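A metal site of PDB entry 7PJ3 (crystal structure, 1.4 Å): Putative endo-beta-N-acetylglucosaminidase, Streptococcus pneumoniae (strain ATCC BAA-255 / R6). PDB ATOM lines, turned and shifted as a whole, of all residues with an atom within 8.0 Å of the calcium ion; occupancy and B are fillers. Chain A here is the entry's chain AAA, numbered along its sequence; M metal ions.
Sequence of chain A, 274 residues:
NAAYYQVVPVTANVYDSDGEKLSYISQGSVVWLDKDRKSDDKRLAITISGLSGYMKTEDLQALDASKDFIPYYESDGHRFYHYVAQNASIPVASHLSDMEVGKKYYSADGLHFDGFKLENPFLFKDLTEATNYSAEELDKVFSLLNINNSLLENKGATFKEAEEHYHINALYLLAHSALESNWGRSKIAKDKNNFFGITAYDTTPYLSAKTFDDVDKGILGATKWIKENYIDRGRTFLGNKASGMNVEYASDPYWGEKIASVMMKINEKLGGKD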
ATOM      1  N   TYR A  15     -15.421  19.612 -27.559  1.00  0.00           N
ATOM      2  CA  TYR A  15     -14.175  19.029 -27.036  1.00  0.00           C
ATOM      3  C   TYR A  15     -12.981  19.838 -27.519  1.00  0.00           C
ATOM      4  O   TYR A  15     -13.048  20.532 -28.528  1.00  0.00           O
ATOM      5  CB  TYR A  15     -14.033  17.580 -27.507  1.00  0.00           C
ATOM      6  CG  TYR A  15     -15.153  16.664 -27.118  1.00  0.00           C
ATOM      7  CD1 TYR A  15     -15.136  16.006 -25.902  1.00  0.00           C
ATOM      8  CD2 TYR A  15     -16.269  16.502 -27.940  1.00  0.00           C
ATOM      9  CE1 TYR A  15     -16.161  15.156 -25.531  1.00  0.00           C
ATOM     10  CE2 TYR A  15     -17.318  15.689 -27.582  1.00  0.00           C
ATOM     11  CZ  TYR A  15     -17.247  14.995 -26.376  1.00  0.00           C
ATOM     12  OH  TYR A  15     -18.299  14.230 -26.034  1.00  0.00           O
ATOM     13  N   ASP A  16     -11.886  19.725 -26.805  1.00  0.00           N
ATOM     14  CA  ASP A  16     -10.587  20.258 -27.259  1.00  0.00           C
ATOM     15  C   ASP A  16      -9.848  19.186 -28.059  1.00  0.00           C
ATOM     16  O   ASP A  16     -10.392  18.089 -28.235  1.00  0.00           O
ATOM     17  CB  ASP A  16      -9.819  20.803 -26.073  1.00  0.00           C
ATOM     18  CG  ASP A  16      -9.140  19.831 -25.164  1.00  0.00           C
ATOM     19  OD1 ASP A  16      -9.216  18.604 -25.446  1.00  0.00           O
ATOM     20  OD2 ASP A  16      -8.503  20.339 -24.222  1.00  0.00           O
ATOM     21  N   SER A  17      -8.658  19.488 -28.515  1.00  0.00           N
ATOM     22  CA  SER A  17      -7.861  18.562 -29.372  1.00  0.00           C
ATOM     23  C   SER A  17      -7.441  17.292 -28.602  1.00  0.00           C
ATOM     24  O   SER A  17      -7.046  16.304 -29.272  1.00  0.00           O
ATOM     25  CB  SER A  17      -6.665  19.266 -29.956  1.00  0.00           C
ATOM     26  OG  SER A  17      -5.828  19.766 -28.935  1.00  0.00           O
ATOM     27  N   ASP A  18      -7.434  17.334 -27.260  1.00  0.00           N
ATOM     28  CA  ASP A  18      -7.081  16.201 -26.366  1.00  0.00           C
ATOM     29  C   ASP A  18      -8.321  15.325 -26.149  1.00  0.00           C
ATOM     30  O   ASP A  18      -8.200  14.276 -25.498  1.00  0.00           O
ATOM     31  CB  ASP A  18      -6.631  16.640 -24.960  1.00  0.00           C
ATOM     32  CG  ASP A  18      -5.424  17.550 -24.875  1.00  0.00           C
ATOM     33  OD1 ASP A  18      -4.518  17.361 -25.697  1.00  0.00           O
ATOM     34  OD2 ASP A  18      -5.397  18.451 -23.934  1.00  0.00           O
ATOM     35  N   GLY A  19      -9.492  15.747 -26.642  1.00  0.00           N
ATOM     36  CA  GLY A  19     -10.760  15.043 -26.366  1.00  0.00           C
ATOM     37  C   GLY A  19     -11.386  15.413 -25.034  1.00  0.00           C
ATOM     38  O   GLY A  19     -12.307  14.699 -24.583  1.00  0.00           O
ATOM     39  N   GLU A  20     -10.882  16.452 -24.376  1.00  0.00           N
ATOM     40  CA  GLU A  20     -11.446  16.916 -23.071  1.00  0.00           C
ATOM     41  C   GLU A  20     -12.674  17.763 -23.386  1.00  0.00           C
ATOM     42  O   GLU A  20     -12.671  18.548 -24.326  1.00  0.00           O
ATOM     43  CB  GLU A  20     -10.406  17.669 -22.260  1.00  0.00           C
ATOM     44  CG  GLU A  20      -9.322  16.775 -21.710  1.00  0.00           C
ATOM     45  CD  GLU A  20      -8.240  17.520 -20.937  1.00  0.00           C
ATOM     46  OE1 GLU A  20      -7.923  18.639 -21.349  1.00  0.00           O
ATOM     47  OE2 GLU A  20      -7.735  16.972 -19.918  1.00  0.00           O
ATOM     48  N   LYS A  21     -13.716  17.596 -22.578  1.00  0.00           N
ATOM     49  CA  LYS A  21     -14.983  18.367 -22.679  1.00  0.00           C
ATOM     50  C   LYS A  21     -14.711  19.818 -22.279  1.00  0.00           C
ATOM     51  O   LYS A  21     -14.223  20.049 -21.155  1.00  0.00           O
ATOM     52  CB  LYS A  21     -16.043  17.722 -21.794  1.00  0.00           C
ATOM     53  CG  LYS A  21     -16.407  16.279 -22.148  1.00  0.00           C
ATOM     54  CD  LYS A  21     -17.471  15.666 -21.247  1.00  0.00           C
ATOM     55  CE  LYS A  21     -17.266  14.188 -21.023  1.00  0.00           C
ATOM     56  NZ  LYS A  21     -17.835  13.747 -19.716  1.00  0.00           N
ATOM     57  N   LEU A  22     -15.024  20.743 -23.176  1.00  0.00           N
ATOM     58  CA  LEU A  22     -14.940  22.213 -22.919  1.00  0.00           C
ATOM     59  C   LEU A  22     -16.293  22.792 -22.522  1.00  0.00           C
ATOM     60  O   LEU A  22     -16.350  23.633 -21.612  1.00  0.00           O
ATOM     61  CB  LEU A  22     -14.454  22.887 -24.194  1.00  0.00           C
ATOM     62  CG  LEU A  22     -13.048  22.485 -24.573  1.00  0.00           C
ATOM     63  CD1 LEU A  22     -12.611  23.229 -25.800  1.00  0.00           C
ATOM     64  CD2 LEU A  22     -12.085  22.673 -23.407  1.00  0.00           C
HETATM   65 CA    CA M   1      -6.897  20.068 -22.598  1.00  0.00          CA
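The side-chain carboxylate (OD1) of Asp 16 is in hydrogen-bond range of the backbone NH (N) of Gly 19 (3.1 Å).
The calcium ion is bound by the side-chain carboxylate of Glu 20 (2.2 Å), the side-chain carboxylate of Asp 16 (2.3 Å) and the side-chain carboxylate of Asp 18 (2.6 Å). The calcium ion has three donor atoms within binding distance.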
